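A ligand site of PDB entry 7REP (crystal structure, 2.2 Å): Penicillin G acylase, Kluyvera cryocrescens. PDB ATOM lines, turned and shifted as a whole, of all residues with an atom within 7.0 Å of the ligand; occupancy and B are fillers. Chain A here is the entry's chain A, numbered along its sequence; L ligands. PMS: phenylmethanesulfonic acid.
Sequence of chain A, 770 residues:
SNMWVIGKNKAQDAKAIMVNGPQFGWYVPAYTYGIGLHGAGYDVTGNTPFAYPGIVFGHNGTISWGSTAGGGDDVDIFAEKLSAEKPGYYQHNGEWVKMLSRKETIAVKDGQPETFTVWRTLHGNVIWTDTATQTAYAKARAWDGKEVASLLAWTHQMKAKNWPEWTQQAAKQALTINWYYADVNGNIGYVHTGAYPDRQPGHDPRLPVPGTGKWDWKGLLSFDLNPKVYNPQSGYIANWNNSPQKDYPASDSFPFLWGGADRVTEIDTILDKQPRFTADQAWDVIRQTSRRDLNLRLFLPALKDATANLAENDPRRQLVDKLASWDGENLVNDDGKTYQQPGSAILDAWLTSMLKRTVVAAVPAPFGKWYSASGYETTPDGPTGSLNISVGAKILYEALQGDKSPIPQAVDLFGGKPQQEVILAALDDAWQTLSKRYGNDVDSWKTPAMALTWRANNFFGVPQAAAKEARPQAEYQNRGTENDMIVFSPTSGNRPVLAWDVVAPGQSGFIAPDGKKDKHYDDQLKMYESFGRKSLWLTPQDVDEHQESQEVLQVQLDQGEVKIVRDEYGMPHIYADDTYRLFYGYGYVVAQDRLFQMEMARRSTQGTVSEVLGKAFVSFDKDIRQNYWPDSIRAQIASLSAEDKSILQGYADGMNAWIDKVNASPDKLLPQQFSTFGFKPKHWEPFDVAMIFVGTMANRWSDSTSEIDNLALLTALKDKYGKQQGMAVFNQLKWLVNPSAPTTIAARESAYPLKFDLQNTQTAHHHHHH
O1S of the ligand sits at hydrogen-bond distance from N of Ala 69 (2.8 Å).
O1S of the ligand sits at hydrogen-bond distance from ND2 of Asn 241 (2.9 Å).
An oxygen (O2S) of the ligand sits close to the backbone NH of Ser 1 (3.4 Å).
OG of Ser 1 is bonded to S of the ligand (1.5 Å).
O of Ala 69 lies within hydrogen-bond range of ND2 of Asn 178.
The side-chain amide oxygen (OE1) of Gln 23 is in hydrogen-bond range of the indole nitrogen (NE1) of Trp 240 (2.8 Å).
N of Asn 241 is in hydrogen-bond range of OD1 of Asn 239, at 3.0 Å.
The backbone carbonyl oxygen of Thr 68 is in hydrogen-bond range of the backbone NH of Asn 178, at 2.8 Å.
N of Gln 23 sits at hydrogen-bond distance from OG of Ser 1 (2.9 Å).
The guanidinium group (NH2) of Arg 263 is in hydrogen-bond range of the side-chain amide oxygen (OD1) of Asn 241 (2.8 Å).
The side-chain amide oxygen (OD1) of Asn 241 sits at hydrogen-bond distance from the backbone NH (N) of Ser 1.
The side-chain amide oxygen (OD1) of Asn 20 sits at hydrogen-bond distance from the backbone NH (N) of Ser 67 (3.2 Å).
O2S of the ligand sits close to O of Gln 23.
CB of Pro 22 touches C2 of the ligand, 3.7 Å away.
CE1 of Phe 24 touches C1 of the ligand, at 3.6 Å.
O of Ser 67 touches C3 of the ligand, 3.5 Å away.
Thr 68 touches the ligand (CA to C2, 3.7 Å).
Met 697 touches the ligand.
CZ3 of Trp 701 touches O2S of the ligand, at 3.5 Å.
Hydrophobic or aromatic side chains within 4 Å of the ligand: Pro 22, Phe 24, Ala 69, Met 697 and Trp 701.
Ten residues have an atom within 4 Å of the ligand: Ser 1, Pro 22, Gln 23, Phe 24, Ser 67, Thr 68, Ala 69, Asn 241, Met 697 and Trp 701.
The nearest printed residue that does not touch the ligand is Ile 177 (4.01 Å).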
ATOM      1  N   SER A   1     -11.906  30.127 -17.635  1.00  0.00           N
ATOM      2  CA  SER A   1     -12.347  30.824 -16.432  1.00  0.00           C
ATOM      3  C   SER A   1     -11.470  32.042 -16.179  1.00  0.00           C
ATOM      4  O   SER A   1     -10.252  31.884 -16.095  1.00  0.00           O
ATOM      5  CB  SER A   1     -12.219  29.915 -15.215  1.00  0.00           C
ATOM      6  OG  SER A   1     -13.136  28.833 -15.248  1.00  0.00           O
ATOM      7  N   ASN A   2     -12.064  33.244 -16.006  1.00  0.00           N
ATOM      8  CA  ASN A   2     -11.243  34.416 -15.750  1.00  0.00           C
ATOM      9  C   ASN A   2     -11.602  35.105 -14.419  1.00  0.00           C
ATOM     10  O   ASN A   2     -12.604  34.793 -13.790  1.00  0.00           O
ATOM     11  CB  ASN A   2     -11.181  35.379 -16.951  1.00  0.00           C
ATOM     12  CG  ASN A   2     -12.494  35.800 -17.548  1.00  0.00           C
ATOM     13  OD1 ASN A   2     -13.513  35.899 -16.851  1.00  0.00           O
ATOM     14  ND2 ASN A   2     -12.488  36.083 -18.858  1.00  0.00           N
ATOM     15  N   ASN A  20     -15.408  37.886 -11.283  1.00  0.00           N
ATOM     16  CA  ASN A  20     -15.159  36.486 -11.603  1.00  0.00           C
ATOM     17  C   ASN A  20     -16.032  35.999 -12.761  1.00  0.00           C
ATOM     18  O   ASN A  20     -17.227  36.214 -12.764  1.00  0.00           O
ATOM     19  CB  ASN A  20     -15.516  35.657 -10.361  1.00  0.00           C
ATOM     20  CG  ASN A  20     -14.800  34.348 -10.144  1.00  0.00           C
ATOM     21  OD1 ASN A  20     -14.839  33.800  -9.038  1.00  0.00           O
ATOM     22  ND2 ASN A  20     -14.082  33.814 -11.141  1.00  0.00           N
ATOM     23  N   GLY A  21     -15.418  35.286 -13.704  1.00  0.00           N
ATOM     24  CA  GLY A  21     -16.144  34.702 -14.823  1.00  0.00           C
ATOM     25  C   GLY A  21     -15.723  33.277 -15.061  1.00  0.00           C
ATOM     26  O   GLY A  21     -14.952  32.996 -15.974  1.00  0.00           O
ATOM     27  N   PRO A  22     -16.167  32.336 -14.223  1.00  0.00           N
ATOM     28  CA  PRO A  22     -15.763  30.931 -14.416  1.00  0.00           C
ATOM     29  C   PRO A  22     -16.423  30.332 -15.668  1.00  0.00           C
ATOM     30  O   PRO A  22     -17.625  30.466 -15.851  1.00  0.00           O
ATOM     31  CB  PRO A  22     -16.251  30.257 -13.138  1.00  0.00           C
ATOM     32  CG  PRO A  22     -17.505  31.051 -12.792  1.00  0.00           C
ATOM     33  CD  PRO A  22     -17.093  32.473 -13.072  1.00  0.00           C
ATOM     34  N   GLN A  23     -15.631  29.645 -16.495  1.00  0.00           N
ATOM     35  CA  GLN A  23     -16.112  29.064 -17.740  1.00  0.00           C
ATOM     36  C   GLN A  23     -16.297  27.555 -17.678  1.00  0.00           C
ATOM     37  O   GLN A  23     -15.346  26.786 -17.757  1.00  0.00           O
ATOM     38  CB  GLN A  23     -15.215  29.474 -18.925  1.00  0.00           C
ATOM     39  CG  GLN A  23     -15.116  30.984 -19.039  1.00  0.00           C
ATOM     40  CD  GLN A  23     -14.344  31.438 -20.251  1.00  0.00           C
ATOM     41  OE1 GLN A  23     -13.115  31.573 -20.227  1.00  0.00           O
ATOM     42  NE2 GLN A  23     -15.056  31.712 -21.333  1.00  0.00           N
ATOM     43  N   PHE A  24     -17.526  27.155 -17.599  1.00  0.00           N
ATOM     44  CA  PHE A  24     -17.935  25.760 -17.496  1.00  0.00           C
ATOM     45  C   PHE A  24     -18.775  25.279 -18.683  1.00  0.00           C
ATOM     46  O   PHE A  24     -19.175  24.121 -18.681  1.00  0.00           O
ATOM     47  CB  PHE A  24     -18.852  25.624 -16.275  1.00  0.00           C
ATOM     48  CG  PHE A  24     -18.281  26.070 -14.952  1.00  0.00           C
ATOM     49  CD1 PHE A  24     -17.321  25.304 -14.302  1.00  0.00           C
ATOM     50  CD2 PHE A  24     -18.789  27.181 -14.298  1.00  0.00           C
ATOM     51  CE1 PHE A  24     -16.869  25.655 -13.031  1.00  0.00           C
ATOM     52  CE2 PHE A  24     -18.345  27.516 -13.019  1.00  0.00           C
ATOM     53  CZ  PHE A  24     -17.369  26.772 -12.405  1.00  0.00           C
ATOM     54  N   PRO A  49     -21.400  26.127  -8.214  1.00  0.00           N
ATOM     55  CA  PRO A  49     -21.733  25.029  -9.147  1.00  0.00           C
ATOM     56  C   PRO A  49     -22.489  23.886  -8.505  1.00  0.00           C
ATOM     57  O   PRO A  49     -22.132  23.496  -7.401  1.00  0.00           O
ATOM     58  CB  PRO A  49     -20.353  24.508  -9.582  1.00  0.00           C
ATOM     59  CG  PRO A  49     -19.399  25.594  -9.302  1.00  0.00           C
ATOM     60  CD  PRO A  49     -19.945  26.372  -8.130  1.00  0.00           C
ATOM     61  N   VAL A  56     -18.744  28.728  -3.918  1.00  0.00           N
ATOM     62  CA  VAL A  56     -17.492  29.021  -4.594  1.00  0.00           C
ATOM     63  C   VAL A  56     -17.380  30.497  -5.014  1.00  0.00           C
ATOM     64  O   VAL A  56     -16.270  31.041  -5.040  1.00  0.00           O
ATOM     65  CB  VAL A  56     -17.349  28.051  -5.812  1.00  0.00           C
ATOM     66  CG1 VAL A  56     -16.068  28.328  -6.585  1.00  0.00           C
ATOM     67  CG2 VAL A  56     -17.396  26.585  -5.360  1.00  0.00           C
ATOM     68  N   PHE A  57     -18.499  31.124  -5.349  1.00  0.00           N
ATOM     69  CA  PHE A  57     -18.458  32.532  -5.800  1.00  0.00           C
ATOM     70  C   PHE A  57     -19.318  33.388  -4.851  1.00  0.00           C
ATOM     71  O   PHE A  57     -20.527  33.259  -4.867  1.00  0.00           O
ATOM     72  CB  PHE A  57     -18.917  32.655  -7.290  1.00  0.00           C
ATOM     73  CG  PHE A  57     -18.329  31.568  -8.199  1.00  0.00           C
ATOM     74  CD1 PHE A  57     -17.003  31.600  -8.561  1.00  0.00           C
ATOM     75  CD2 PHE A  57     -19.091  30.489  -8.596  1.00  0.00           C
ATOM     76  CE1 PHE A  57     -16.461  30.597  -9.353  1.00  0.00           C
ATOM     77  CE2 PHE A  57     -18.538  29.479  -9.390  1.00  0.00           C
ATOM     78  CZ  PHE A  57     -17.224  29.532  -9.748  1.00  0.00           C
ATOM     79  N   GLY A  66     -13.338  33.915  -4.816  1.00  0.00           N
ATOM     80  CA  GLY A  66     -13.692  33.290  -6.075  1.00  0.00           C
ATOM     81  C   GLY A  66     -12.620  32.322  -6.518  1.00  0.00           C
ATOM     82  O   GLY A  66     -11.566  32.208  -5.872  1.00  0.00           O
ATOM     83  N   SER A  67     -12.873  31.633  -7.650  1.00  0.00           N
ATOM     84  CA  SER A  67     -11.848  30.725  -8.156  1.00  0.00           C
ATOM     85  C   SER A  67     -11.892  30.501  -9.682  1.00  0.00           C
ATOM     86  O   SER A  67     -12.836  30.891 -10.358  1.00  0.00           O
ATOM     87  CB  SER A  67     -11.867  29.401  -7.390  1.00  0.00           C
ATOM     88  OG  SER A  67     -13.117  28.749  -7.460  1.00  0.00           O
ATOM     89  N   THR A  68     -10.765  29.990 -10.207  1.00  0.00           N
ATOM     90  CA  THR A  68     -10.498  29.499 -11.568  1.00  0.00           C
ATOM     91  C   THR A  68      -9.721  28.163 -11.392  1.00  0.00           C
ATOM     92  O   THR A  68      -9.152  27.923 -10.325  1.00  0.00           O
ATOM     93  CB  THR A  68      -9.739  30.511 -12.430  1.00  0.00           C
ATOM     94  OG1 THR A  68      -8.437  30.698 -11.921  1.00  0.00           O
ATOM     95  CG2 THR A  68     -10.448  31.873 -12.543  1.00  0.00           C
ATOM     96  N   ALA A  69      -9.702  27.295 -12.413  1.00  0.00           N
ATOM     97  CA  ALA A  69      -8.976  26.016 -12.313  1.00  0.00           C
ATOM     98  C   ALA A  69      -7.506  26.301 -12.280  1.00  0.00           C
ATOM     99  O   ALA A  69      -7.029  27.198 -12.963  1.00  0.00           O
ATOM    100  CB  ALA A  69      -9.340  25.092 -13.478  1.00  0.00           C
ATOM    101  N   GLY A  70      -6.792  25.598 -11.404  1.00  0.00           N
ATOM    102  CA  GLY A  70      -5.374  25.820 -11.166  1.00  0.00           C
ATOM    103  C   GLY A  70      -4.456  25.419 -12.291  1.00  0.00           C
ATOM    104  O   GLY A  70      -3.469  26.114 -12.558  1.00  0.00           O
ATOM    105  N   TRP A 154     -13.904  24.526   1.396  1.00  0.00           N
ATOM    106  CA  TRP A 154     -14.655  25.519   0.617  1.00  0.00           C
ATOM    107  C   TRP A 154     -15.847  26.033   1.414  1.00  0.00           C
ATOM    108  O   TRP A 154     -16.271  27.173   1.226  1.00  0.00           O
ATOM    109  CB  TRP A 154     -15.168  24.906  -0.691  1.00  0.00           C
ATOM    110  CG  TRP A 154     -14.665  25.614  -1.917  1.00  0.00           C
ATOM    111  CD1 TRP A 154     -14.846  26.927  -2.255  1.00  0.00           C
ATOM    112  CD2 TRP A 154     -13.949  25.019  -3.007  1.00  0.00           C
ATOM    113  NE1 TRP A 154     -14.263  27.188  -3.467  1.00  0.00           N
ATOM    114  CE2 TRP A 154     -13.692  26.039  -3.952  1.00  0.00           C
ATOM    115  CE3 TRP A 154     -13.463  23.723  -3.268  1.00  0.00           C
ATOM    116  CZ2 TRP A 154     -12.996  25.794  -5.140  1.00  0.00           C
ATOM    117  CZ3 TRP A 154     -12.759  23.488  -4.430  1.00  0.00           C
ATOM    118  CH2 TRP A 154     -12.555  24.512  -5.368  1.00  0.00           C
ATOM    119  N   THR A 176      -6.307  21.120  -7.524  1.00  0.00           N
ATOM    120  CA  THR A 176      -5.528  22.169  -8.162  1.00  0.00           C
ATOM    121  C   THR A 176      -6.471  23.293  -8.607  1.00  0.00           C
ATOM    122  O   THR A 176      -7.067  23.223  -9.681  1.00  0.00           O
ATOM    123  CB  THR A 176      -4.589  21.621  -9.269  1.00  0.00           C
ATOM    124  OG1 THR A 176      -3.741  22.673  -9.724  1.00  0.00           O
ATOM    125  CG2 THR A 176      -5.316  20.935 -10.420  1.00  0.00           C
ATOM    126  N   ILE A 177      -6.701  24.270  -7.704  1.00  0.00           N
ATOM    127  CA  ILE A 177      -7.635  25.375  -7.901  1.00  0.00           C
ATOM    128  C   ILE A 177      -7.015  26.709  -7.471  1.00  0.00           C
ATOM    129  O   ILE A 177      -6.342  26.771  -6.458  1.00  0.00           O
ATOM    130  CB  ILE A 177      -8.941  25.111  -7.125  1.00  0.00           C
ATOM    131  CG1 ILE A 177      -9.526  23.706  -7.405  1.00  0.00           C
ATOM    132  CG2 ILE A 177      -9.989  26.206  -7.370  1.00  0.00           C
ATOM    133  CD1 ILE A 177     -10.151  23.525  -8.806  1.00  0.00           C
ATOM    134  N   ASN A 178      -7.217  27.760  -8.277  1.00  0.00           N
ATOM    135  CA  ASN A 178      -6.748  29.083  -7.930  1.00  0.00           C
ATOM    136  C   ASN A 178      -7.840  29.696  -7.068  1.00  0.00           C
ATOM    137  O   ASN A 178      -9.007  29.644  -7.434  1.00  0.00           O
ATOM    138  CB  ASN A 178      -6.612  29.905  -9.171  1.00  0.00           C
ATOM    139  CG  ASN A 178      -5.417  29.539  -9.986  1.00  0.00           C
ATOM    140  OD1 ASN A 178      -4.346  29.282  -9.455  1.00  0.00           O
ATOM    141  ND2 ASN A 178      -5.593  29.519 -11.288  1.00  0.00           N
ATOM    142  N   ASN A 239      -6.263  36.535 -13.869  1.00  0.00           N
ATOM    143  CA  ASN A 239      -6.041  35.161 -14.326  1.00  0.00           C
ATOM    144  C   ASN A 239      -7.033  34.724 -15.427  1.00  0.00           C
ATOM    145  O   ASN A 239      -8.212  35.067 -15.381  1.00  0.00           O
ATOM    146  CB  ASN A 239      -6.106  34.182 -13.156  1.00  0.00           C
ATOM    147  CG  ASN A 239      -5.771  32.736 -13.486  1.00  0.00           C
ATOM    148  OD1 ASN A 239      -6.632  31.918 -13.827  1.00  0.00           O
ATOM    149  ND2 ASN A 239      -4.497  32.355 -13.358  1.00  0.00           N
ATOM    150  N   TRP A 240      -6.576  33.926 -16.367  1.00  0.00           N
ATOM    151  CA  TRP A 240      -7.440  33.334 -17.393  1.00  0.00           C
ATOM    152  C   TRP A 240      -6.830  31.985 -17.735  1.00  0.00           C
ATOM    153  O   TRP A 240      -6.493  31.725 -18.900  1.00  0.00           O
ATOM    154  CB  TRP A 240      -7.605  34.228 -18.647  1.00  0.00           C
ATOM    155  CG  TRP A 240      -8.860  33.962 -19.448  1.00  0.00           C
ATOM    156  CD1 TRP A 240      -9.721  32.910 -19.328  1.00  0.00           C
ATOM    157  CD2 TRP A 240      -9.377  34.774 -20.522  1.00  0.00           C
ATOM    158  NE1 TRP A 240     -10.755  33.035 -20.214  1.00  0.00           N
ATOM    159  CE2 TRP A 240     -10.571  34.167 -20.966  1.00  0.00           C
ATOM    160  CE3 TRP A 240      -8.966  35.969 -21.117  1.00  0.00           C
ATOM    161  CZ2 TRP A 240     -11.349  34.715 -21.984  1.00  0.00           C
ATOM    162  CZ3 TRP A 240      -9.744  36.500 -22.120  1.00  0.00           C
ATOM    163  CH2 TRP A 240     -10.917  35.882 -22.543  1.00  0.00           C
ATOM    164  N   ASN A 241      -6.652  31.146 -16.687  1.00  0.00           N
ATOM    165  CA  ASN A 241      -6.038  29.816 -16.715  1.00  0.00           C
ATOM    166  C   ASN A 241      -4.565  29.857 -17.094  1.00  0.00           C
ATOM    167  O   ASN A 241      -4.019  28.854 -17.557  1.00  0.00           O
ATOM    168  CB  ASN A 241      -6.823  28.800 -17.547  1.00  0.00           C
ATOM    169  CG  ASN A 241      -8.275  28.735 -17.149  1.00  0.00           C
ATOM    170  OD1 ASN A 241      -9.160  29.188 -17.884  1.00  0.00           O
ATOM    171  ND2 ASN A 241      -8.572  28.215 -15.966  1.00  0.00           N
ATOM    172  N   ARG A 263      -3.761  34.033 -23.295  1.00  0.00           N
ATOM    173  CA  ARG A 263      -4.924  34.915 -23.350  1.00  0.00           C
ATOM    174  C   ARG A 263      -5.058  35.832 -22.154  1.00  0.00           C
ATOM    175  O   ARG A 263      -5.780  36.819 -22.269  1.00  0.00           O
ATOM    176  CB  ARG A 263      -6.219  34.138 -23.603  1.00  0.00           C
ATOM    177  CG  ARG A 263      -6.624  33.279 -22.438  1.00  0.00           C
ATOM    178  CD  ARG A 263      -7.835  32.430 -22.752  1.00  0.00           C
ATOM    179  NE  ARG A 263      -8.107  31.529 -21.643  1.00  0.00           N
ATOM    180  CZ  ARG A 263      -9.008  30.554 -21.666  1.00  0.00           C
ATOM    181  NH1 ARG A 263      -9.746  30.352 -22.747  1.00  0.00           N
ATOM    182  NH2 ARG A 263      -9.174  29.774 -20.605  1.00  0.00           N
ATOM    183  N   SER A 386     -14.738  27.770 -23.546  1.00  0.00           N
ATOM    184  CA  SER A 386     -14.084  29.045 -23.845  1.00  0.00           C
ATOM    185  C   SER A 386     -13.315  28.954 -25.186  1.00  0.00           C
ATOM    186  O   SER A 386     -13.069  27.870 -25.721  1.00  0.00           O
ATOM    187  CB  SER A 386     -13.114  29.405 -22.724  1.00  0.00           C
ATOM    188  OG  SER A 386     -11.949  28.593 -22.766  1.00  0.00           O
ATOM    189  N   MET A 697     -16.205  18.481  -9.599  1.00  0.00           N
ATOM    190  CA  MET A 697     -15.152  19.433  -9.322  1.00  0.00           C
ATOM    191  C   MET A 697     -13.803  18.741  -9.366  1.00  0.00           C
ATOM    192  O   MET A 697     -12.927  19.184 -10.092  1.00  0.00           O
ATOM    193  CB  MET A 697     -15.384  20.110  -7.948  1.00  0.00           C
ATOM    194  CG  MET A 697     -15.591  21.610  -8.026  1.00  0.00           C
ATOM    195  SD  MET A 697     -14.209  22.582  -8.648  1.00  0.00           S
ATOM    196  CE  MET A 697     -12.974  21.912  -7.710  1.00  0.00           C
ATOM    197  N   TRP A 701     -11.998  19.276 -12.980  1.00  0.00           N
ATOM    198  CA  TRP A 701     -10.956  20.285 -12.998  1.00  0.00           C
ATOM    199  C   TRP A 701      -9.652  19.911 -12.345  1.00  0.00           C
ATOM    200  O   TRP A 701      -8.688  20.674 -12.480  1.00  0.00           O
ATOM    201  CB  TRP A 701     -11.519  21.574 -12.379  1.00  0.00           C
ATOM    202  CG  TRP A 701     -12.792  22.024 -13.047  1.00  0.00           C
ATOM    203  CD1 TRP A 701     -14.056  21.858 -12.582  1.00  0.00           C
ATOM    204  CD2 TRP A 701     -12.908  22.552 -14.373  1.00  0.00           C
ATOM    205  NE1 TRP A 701     -14.963  22.352 -13.491  1.00  0.00           N
ATOM    206  CE2 TRP A 701     -14.283  22.753 -14.630  1.00  0.00           C
ATOM    207  CE3 TRP A 701     -11.996  22.863 -15.384  1.00  0.00           C
ATOM    208  CZ2 TRP A 701     -14.754  23.267 -15.833  1.00  0.00           C
ATOM    209  CZ3 TRP A 701     -12.459  23.376 -16.581  1.00  0.00           C
ATOM    210  CH2 TRP A 701     -13.818  23.583 -16.790  1.00  0.00           C
HETATM  211  C   PMS L   1     -13.671  27.038 -14.439  1.00  0.00           C
HETATM  212  S   PMS L   1     -12.327  27.625 -15.541  1.00  0.00           S
HETATM  213  C1  PMS L   1     -13.418  26.831 -12.964  1.00  0.00           C
HETATM  214  C2  PMS L   1     -13.778  27.786 -12.035  1.00  0.00           C
HETATM  215  C3  PMS L   1     -13.642  27.548 -10.677  1.00  0.00           C
HETATM  216  C4  PMS L   1     -13.194  26.320 -10.218  1.00  0.00           C
HETATM  217  C5  PMS L   1     -12.854  25.356 -11.137  1.00  0.00           C
HETATM  218  C6  PMS L   1     -12.990  25.594 -12.495  1.00  0.00           C
HETATM  219  O2S PMS L   1     -12.414  26.855 -16.748  1.00  0.00           O
HETATM  220  O1S PMS L   1     -11.110  27.543 -14.807  1.00  0.00           O
